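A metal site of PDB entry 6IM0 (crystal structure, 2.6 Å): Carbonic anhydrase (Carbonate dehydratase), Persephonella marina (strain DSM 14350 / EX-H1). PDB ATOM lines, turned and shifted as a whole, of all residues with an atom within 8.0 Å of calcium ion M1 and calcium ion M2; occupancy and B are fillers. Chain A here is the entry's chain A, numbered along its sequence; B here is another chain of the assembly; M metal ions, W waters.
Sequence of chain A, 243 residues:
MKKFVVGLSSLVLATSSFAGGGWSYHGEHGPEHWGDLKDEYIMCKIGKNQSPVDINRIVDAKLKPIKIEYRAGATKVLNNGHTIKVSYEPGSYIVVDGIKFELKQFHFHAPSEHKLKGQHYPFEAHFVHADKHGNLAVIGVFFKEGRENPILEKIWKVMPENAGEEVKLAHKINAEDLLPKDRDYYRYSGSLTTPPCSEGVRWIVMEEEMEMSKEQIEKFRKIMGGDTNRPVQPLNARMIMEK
The backbone carbonyl oxygen of Glu 242 of chain B lies within hydrogen-bond range of the backbone NH of Ala 61 of chain B (3.0 Å).
The backbone NH of Glu 242 of chain B lies within hydrogen-bond range of the backbone carbonyl oxygen of Val 59 of chain B, at 2.9 Å.
Of the 22 residues printed, 4 come within 4 Å of calcium ion M1.
Of the 22 residues printed, 3 come within 4 Å of calcium ion M2.
Calcium ion M1 is bound by the side-chain carboxylate (OD1) of Asp 60 of chain B (2.2 Å), the side-chain carboxylate (OE2) of Glu 208 (2.5 Å), the side-chain carboxylate (OE1) of Glu 209 (2.5 Å), the side-chain carboxylate (OE1) of Glu 242 of chain B (2.5 Å), the side-chain carboxylate (OE1) of Glu 208 (2.6 Å), the side-chain carboxylate (OE2) of Glu 209 (2.6 Å) and water W1 (2.8 Å).
Calcium ion M1 has seven donor atoms within binding distance.
Slightly farther from calcium ion M1 lies OE2 of Glu 242 of chain B (3.1 Å).
Calcium ion M2 is bound by OD2 of Asp 60 of chain B (2.2 Å), O of Glu 209 (2.3 Å), OE2 of Glu 208 (2.5 Å), water W2 (2.5 Å) and OE2 of Glu 209 (2.7 Å).
Calcium ion M2 has five donor atoms within binding distance.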
ATOM      1  N   TYR A 121       3.236   3.237   4.422  1.00  0.00           N
ATOM      2  CA  TYR A 121       3.463   1.885   3.896  1.00  0.00           C
ATOM      3  C   TYR A 121       3.397   0.936   5.103  1.00  0.00           C
ATOM      4  O   TYR A 121       3.574   1.381   6.229  1.00  0.00           O
ATOM      5  CB  TYR A 121       4.836   1.787   3.240  1.00  0.00           C
ATOM      6  CG  TYR A 121       4.959   2.484   1.893  1.00  0.00           C
ATOM      7  CD1 TYR A 121       5.233   3.850   1.807  1.00  0.00           C
ATOM      8  CD2 TYR A 121       4.838   1.760   0.697  1.00  0.00           C
ATOM      9  CE1 TYR A 121       5.367   4.474   0.579  1.00  0.00           C
ATOM     10  CE2 TYR A 121       4.986   2.381  -0.523  1.00  0.00           C
ATOM     11  CZ  TYR A 121       5.236   3.752  -0.576  1.00  0.00           C
ATOM     12  OH  TYR A 121       5.373   4.353  -1.795  1.00  0.00           O
ATOM     13  N   PHE A 142      10.933   1.941   1.779  1.00  0.00           N
ATOM     14  CA  PHE A 142       9.561   1.524   2.016  1.00  0.00           C
ATOM     15  C   PHE A 142       9.347   0.143   1.432  1.00  0.00           C
ATOM     16  O   PHE A 142       9.895  -0.209   0.389  1.00  0.00           O
ATOM     17  CB  PHE A 142       8.577   2.445   1.332  1.00  0.00           C
ATOM     18  CG  PHE A 142       8.551   3.841   1.879  1.00  0.00           C
ATOM     19  CD1 PHE A 142       8.209   4.064   3.222  1.00  0.00           C
ATOM     20  CD2 PHE A 142       8.805   4.940   1.068  1.00  0.00           C
ATOM     21  CE1 PHE A 142       8.141   5.353   3.721  1.00  0.00           C
ATOM     22  CE2 PHE A 142       8.751   6.226   1.576  1.00  0.00           C
ATOM     23  CZ  PHE A 142       8.427   6.438   2.897  1.00  0.00           C
ATOM     24  N   PHE A 143       8.525  -0.656   2.091  1.00  0.00           N
ATOM     25  CA  PHE A 143       8.122  -1.946   1.537  1.00  0.00           C
ATOM     26  C   PHE A 143       6.598  -2.035   1.512  1.00  0.00           C
ATOM     27  O   PHE A 143       5.962  -1.737   2.512  1.00  0.00           O
ATOM     28  CB  PHE A 143       8.631  -3.069   2.394  1.00  0.00           C
ATOM     29  CG  PHE A 143      10.083  -3.407   2.239  1.00  0.00           C
ATOM     30  CD1 PHE A 143      11.065  -2.586   2.760  1.00  0.00           C
ATOM     31  CD2 PHE A 143      10.485  -4.579   1.629  1.00  0.00           C
ATOM     32  CE1 PHE A 143      12.410  -2.901   2.645  1.00  0.00           C
ATOM     33  CE2 PHE A 143      11.832  -4.916   1.503  1.00  0.00           C
ATOM     34  CZ  PHE A 143      12.805  -4.064   2.016  1.00  0.00           C
ATOM     35  N   LYS A 144       6.041  -2.486   0.393  1.00  0.00           N
ATOM     36  CA  LYS A 144       4.608  -2.797   0.305  1.00  0.00           C
ATOM     37  C   LYS A 144       4.357  -4.312   0.355  1.00  0.00           C
ATOM     38  O   LYS A 144       5.283  -5.109   0.193  1.00  0.00           O
ATOM     39  CB  LYS A 144       4.006  -2.191  -0.974  1.00  0.00           C
ATOM     40  CG  LYS A 144       4.548  -2.753  -2.281  1.00  0.00           C
ATOM     41  CD  LYS A 144       3.632  -2.383  -3.442  1.00  0.00           C
ATOM     42  CE  LYS A 144       4.240  -2.829  -4.764  1.00  0.00           C
ATOM     43  NZ  LYS A 144       3.389  -2.488  -5.943  1.00  0.00           N
ATOM     44  N   PRO A 180      16.229  -0.740  -3.929  1.00  0.00           N
ATOM     45  CA  PRO A 180      15.762  -0.720  -5.300  1.00  0.00           C
ATOM     46  C   PRO A 180      16.860  -0.444  -6.316  1.00  0.00           C
ATOM     47  O   PRO A 180      17.941   0.037  -5.961  1.00  0.00           O
ATOM     48  CB  PRO A 180      14.718   0.383  -5.302  1.00  0.00           C
ATOM     49  CG  PRO A 180      15.106   1.275  -4.180  1.00  0.00           C
ATOM     50  CD  PRO A 180      15.698   0.395  -3.146  1.00  0.00           C
ATOM     51  N   LYS A 181      16.565  -0.763  -7.569  1.00  0.00           N
ATOM     52  CA  LYS A 181      17.446  -0.463  -8.694  1.00  0.00           C
ATOM     53  C   LYS A 181      17.276   0.980  -9.177  1.00  0.00           C
ATOM     54  O   LYS A 181      18.258   1.587  -9.574  1.00  0.00           O
ATOM     55  CB  LYS A 181      17.227  -1.470  -9.834  1.00  0.00           C
ATOM     56  CG  LYS A 181      18.095  -2.723  -9.677  1.00  0.00           C
ATOM     57  CD  LYS A 181      17.392  -4.029 -10.082  1.00  0.00           C
ATOM     58  CE  LYS A 181      18.378  -5.207 -10.216  1.00  0.00           C
ATOM     59  NZ  LYS A 181      19.282  -5.408  -9.030  1.00  0.00           N
ATOM     60  N   ASP A 182      16.035   1.525  -9.159  1.00  0.00           N
ATOM     61  CA  ASP A 182      15.780   2.981  -9.282  1.00  0.00           C
ATOM     62  C   ASP A 182      16.282   3.560  -7.955  1.00  0.00           C
ATOM     63  O   ASP A 182      15.738   3.268  -6.892  1.00  0.00           O
ATOM     64  CB  ASP A 182      14.261   3.295  -9.522  1.00  0.00           C
ATOM     65  CG  ASP A 182      13.979   4.783  -9.984  1.00  0.00           C
ATOM     66  OD1 ASP A 182      14.943   5.546 -10.246  1.00  0.00           O
ATOM     67  OD2 ASP A 182      12.784   5.195 -10.174  1.00  0.00           O
ATOM     68  N   GLU A 207      12.595   6.654  -3.239  1.00  0.00           N
ATOM     69  CA  GLU A 207      11.245   6.829  -3.820  1.00  0.00           C
ATOM     70  C   GLU A 207      10.599   5.511  -4.210  1.00  0.00           C
ATOM     71  O   GLU A 207       9.414   5.351  -4.028  1.00  0.00           O
ATOM     72  CB  GLU A 207      11.257   7.710  -5.063  1.00  0.00           C
ATOM     73  CG  GLU A 207      11.803   9.106  -4.822  1.00  0.00           C
ATOM     74  CD  GLU A 207      11.852   9.965  -6.079  1.00  0.00           C
ATOM     75  OE1 GLU A 207      12.825  10.748  -6.231  1.00  0.00           O
ATOM     76  OE2 GLU A 207      10.902   9.844  -6.904  1.00  0.00           O
ATOM     77  N   GLU A 208      11.382   4.591  -4.743  1.00  0.00           N
ATOM     78  CA  GLU A 208      10.848   3.322  -5.143  1.00  0.00           C
ATOM     79  C   GLU A 208      10.784   2.365  -3.967  1.00  0.00           C
ATOM     80  O   GLU A 208      11.780   2.107  -3.263  1.00  0.00           O
ATOM     81  CB  GLU A 208      11.642   2.722  -6.315  1.00  0.00           C
ATOM     82  CG  GLU A 208      11.164   1.368  -6.833  1.00  0.00           C
ATOM     83  CD  GLU A 208       9.711   1.334  -7.276  1.00  0.00           C
ATOM     84  OE1 GLU A 208       9.136   2.365  -7.666  1.00  0.00           O
ATOM     85  OE2 GLU A 208       9.113   0.240  -7.225  1.00  0.00           O
ATOM     86  N   GLU A 209       9.593   1.831  -3.770  1.00  0.00           N
ATOM     87  CA  GLU A 209       9.331   0.828  -2.736  1.00  0.00           C
ATOM     88  C   GLU A 209       9.804  -0.553  -3.135  1.00  0.00           C
ATOM     89  O   GLU A 209       9.922  -0.873  -4.327  1.00  0.00           O
ATOM     90  CB  GLU A 209       7.824   0.795  -2.410  1.00  0.00           C
ATOM     91  CG  GLU A 209       6.945  -0.071  -3.334  1.00  0.00           C
ATOM     92  CD  GLU A 209       6.975   0.314  -4.797  1.00  0.00           C
ATOM     93  OE1 GLU A 209       6.893   1.515  -5.112  1.00  0.00           O
ATOM     94  OE2 GLU A 209       7.115  -0.602  -5.659  1.00  0.00           O
ATOM     95  N   MET A 210       9.986  -1.397  -2.131  1.00  0.00           N
ATOM     96  CA  MET A 210      10.320  -2.813  -2.326  1.00  0.00           C
ATOM     97  C   MET A 210       9.122  -3.612  -1.862  1.00  0.00           C
ATOM     98  O   MET A 210       8.136  -3.032  -1.396  1.00  0.00           O
ATOM     99  CB  MET A 210      11.551  -3.178  -1.517  1.00  0.00           C
ATOM    100  CG  MET A 210      12.832  -2.491  -2.001  1.00  0.00           C
ATOM    101  SD  MET A 210      13.337  -2.916  -3.674  1.00  0.00           S
ATOM    102  CE  MET A 210      14.264  -4.427  -3.396  1.00  0.00           C
ATOM    103  N   GLU A 211       9.210  -4.940  -2.002  1.00  0.00           N
ATOM    104  CA  GLU A 211       8.093  -5.829  -1.697  1.00  0.00           C
ATOM    105  C   GLU A 211       8.429  -6.842  -0.620  1.00  0.00           C
ATOM    106  O   GLU A 211       9.554  -7.283  -0.485  1.00  0.00           O
ATOM    107  CB  GLU A 211       7.698  -6.633  -2.928  1.00  0.00           C
ATOM    108  CG  GLU A 211       6.878  -5.900  -3.972  1.00  0.00           C
ATOM    109  CD  GLU A 211       6.341  -6.854  -5.061  1.00  0.00           C
ATOM    110  OE1 GLU A 211       7.136  -7.725  -5.503  1.00  0.00           O
ATOM    111  OE2 GLU A 211       5.142  -6.739  -5.456  1.00  0.00           O
ATOM    112  N   ILE B  58      -1.138  -0.578  -8.419  1.00  0.00           N
ATOM    113  CA  ILE B  58       0.044  -0.304  -9.172  1.00  0.00           C
ATOM    114  C   ILE B  58       0.950  -1.501  -9.118  1.00  0.00           C
ATOM    115  O   ILE B  58       1.166  -2.077  -8.053  1.00  0.00           O
ATOM    116  CB  ILE B  58       0.785   0.929  -8.591  1.00  0.00           C
ATOM    117  CG1 ILE B  58      -0.185   2.125  -8.559  1.00  0.00           C
ATOM    118  CG2 ILE B  58       1.994   1.276  -9.436  1.00  0.00           C
ATOM    119  CD1 ILE B  58       0.312   3.339  -7.763  1.00  0.00           C
ATOM    120  N   VAL B  59       1.568  -1.825 -10.238  1.00  0.00           N
ATOM    121  CA  VAL B  59       2.586  -2.850 -10.232  1.00  0.00           C
ATOM    122  C   VAL B  59       3.799  -2.424 -10.985  1.00  0.00           C
ATOM    123  O   VAL B  59       3.706  -1.853 -12.042  1.00  0.00           O
ATOM    124  CB  VAL B  59       2.004  -4.175 -10.769  1.00  0.00           C
ATOM    125  CG1 VAL B  59       1.627  -4.044 -12.198  1.00  0.00           C
ATOM    126  CG2 VAL B  59       2.976  -5.327 -10.580  1.00  0.00           C
ATOM    127  N   ASP B  60       4.962  -2.661 -10.408  1.00  0.00           N
ATOM    128  CA  ASP B  60       6.225  -2.353 -11.067  1.00  0.00           C
ATOM    129  C   ASP B  60       6.323  -3.218 -12.316  1.00  0.00           C
ATOM    130  O   ASP B  60       5.957  -4.398 -12.310  1.00  0.00           O
ATOM    131  CB  ASP B  60       7.421  -2.631 -10.132  1.00  0.00           C
ATOM    132  CG  ASP B  60       7.396  -1.804  -8.871  1.00  0.00           C
ATOM    133  OD1 ASP B  60       6.999  -0.614  -8.904  1.00  0.00           O
ATOM    134  OD2 ASP B  60       7.785  -2.329  -7.791  1.00  0.00           O
ATOM    135  N   ALA B  61       6.748  -2.619 -13.403  1.00  0.00           N
ATOM    136  CA  ALA B  61       6.894  -3.321 -14.674  1.00  0.00           C
ATOM    137  C   ALA B  61       8.040  -2.743 -15.479  1.00  0.00           C
ATOM    138  O   ALA B  61       8.302  -1.541 -15.415  1.00  0.00           O
ATOM    139  CB  ALA B  61       5.618  -3.213 -15.463  1.00  0.00           C
ATOM    140  N   LYS B 117      -3.299   7.495  -5.922  1.00  0.00           N
ATOM    141  CA  LYS B 117      -3.546   6.910  -4.611  1.00  0.00           C
ATOM    142  C   LYS B 117      -4.562   7.744  -3.827  1.00  0.00           C
ATOM    143  O   LYS B 117      -4.335   8.149  -2.707  1.00  0.00           O
ATOM    144  CB  LYS B 117      -2.217   6.697  -3.869  1.00  0.00           C
ATOM    145  CG  LYS B 117      -1.554   5.405  -4.295  1.00  0.00           C
ATOM    146  CD  LYS B 117      -0.199   5.157  -3.656  1.00  0.00           C
ATOM    147  CE  LYS B 117       0.157   3.672  -3.694  1.00  0.00           C
ATOM    148  NZ  LYS B 117       1.634   3.461  -3.589  1.00  0.00           N
ATOM    149  N   TYR B 186       3.343   5.877 -15.612  1.00  0.00           N
ATOM    150  CA  TYR B 186       2.316   4.867 -15.448  1.00  0.00           C
ATOM    151  C   TYR B 186       1.660   4.559 -16.786  1.00  0.00           C
ATOM    152  O   TYR B 186       1.401   5.456 -17.571  1.00  0.00           O
ATOM    153  CB  TYR B 186       1.220   5.349 -14.511  1.00  0.00           C
ATOM    154  CG  TYR B 186       1.722   5.733 -13.136  1.00  0.00           C
ATOM    155  CD1 TYR B 186       2.173   4.774 -12.251  1.00  0.00           C
ATOM    156  CD2 TYR B 186       1.743   7.075 -12.725  1.00  0.00           C
ATOM    157  CE1 TYR B 186       2.632   5.152 -11.003  1.00  0.00           C
ATOM    158  CE2 TYR B 186       2.181   7.451 -11.465  1.00  0.00           C
ATOM    159  CZ  TYR B 186       2.628   6.492 -10.620  1.00  0.00           C
ATOM    160  OH  TYR B 186       3.078   6.865  -9.381  1.00  0.00           O
ATOM    161  N   GLU B 207       4.940  10.193 -14.110  1.00  0.00           N
ATOM    162  CA  GLU B 207       5.043  10.156 -12.633  1.00  0.00           C
ATOM    163  C   GLU B 207       5.404  11.492 -12.074  1.00  0.00           C
ATOM    164  O   GLU B 207       4.936  11.871 -11.018  1.00  0.00           O
ATOM    165  CB  GLU B 207       6.057   9.127 -12.144  1.00  0.00           C
ATOM    166  CG  GLU B 207       5.741   7.689 -12.539  1.00  0.00           C
ATOM    167  CD  GLU B 207       6.788   6.681 -12.063  1.00  0.00           C
ATOM    168  OE1 GLU B 207       7.078   5.713 -12.840  1.00  0.00           O
ATOM    169  OE2 GLU B 207       7.306   6.844 -10.925  1.00  0.00           O
ATOM    170  N   MET B 241       0.535  -0.122 -14.602  1.00  0.00           N
ATOM    171  CA  MET B 241       1.930  -0.419 -14.691  1.00  0.00           C
ATOM    172  C   MET B 241       2.810   0.806 -14.375  1.00  0.00           C
ATOM    173  O   MET B 241       2.546   1.886 -14.804  1.00  0.00           O
ATOM    174  CB  MET B 241       2.221  -0.971 -16.064  1.00  0.00           C
ATOM    175  CG  MET B 241       1.790  -2.399 -16.317  1.00  0.00           C
ATOM    176  SD  MET B 241       1.509  -2.672 -18.042  1.00  0.00           S
ATOM    177  CE  MET B 241       2.460  -4.097 -18.368  1.00  0.00           C
ATOM    178  N   GLU B 242       3.872   0.620 -13.606  1.00  0.00           N
ATOM    179  CA  GLU B 242       4.774   1.689 -13.244  1.00  0.00           C
ATOM    180  C   GLU B 242       6.178   1.353 -13.676  1.00  0.00           C
ATOM    181  O   GLU B 242       6.768   0.341 -13.247  1.00  0.00           O
ATOM    182  CB  GLU B 242       4.790   1.902 -11.715  1.00  0.00           C
ATOM    183  CG  GLU B 242       5.688   3.058 -11.291  1.00  0.00           C
ATOM    184  CD  GLU B 242       6.095   3.051  -9.823  1.00  0.00           C
ATOM    185  OE1 GLU B 242       5.288   2.604  -8.959  1.00  0.00           O
ATOM    186  OE2 GLU B 242       7.240   3.518  -9.535  1.00  0.00           O
ATOM    187  N   LYS B 243       6.777   2.264 -14.413  1.00  0.00           N
ATOM    188  CA  LYS B 243       8.151   2.100 -14.850  1.00  0.00           C
ATOM    189  C   LYS B 243       9.212   2.235 -13.744  1.00  0.00           C
ATOM    190  O   LYS B 243       9.233   3.239 -12.987  1.00  0.00           O
ATOM    191  CB  LYS B 243       8.396   3.099 -15.973  1.00  0.00           C
ATOM    192  CG  LYS B 243       9.683   2.844 -16.724  1.00  0.00           C
ATOM    193  CD  LYS B 243       9.857   3.800 -17.891  1.00  0.00           C
ATOM    194  CE  LYS B 243      11.132   3.526 -18.652  1.00  0.00           C
ATOM    195  NZ  LYS B 243      12.345   3.880 -17.879  1.00  0.00           N
HETATM  196 CA    CA M   1       6.872   1.183  -7.597  1.00  0.00          CA
HETATM  197 CA    CA M   2       9.296  -1.999  -6.234  1.00  0.00          CA
HETATM  198  O   HOH W   1       4.244   0.325  -7.216  1.00  0.00           O
HETATM  199  O   HOH W   2       9.183  -4.386  -5.487  1.00  0.00           O
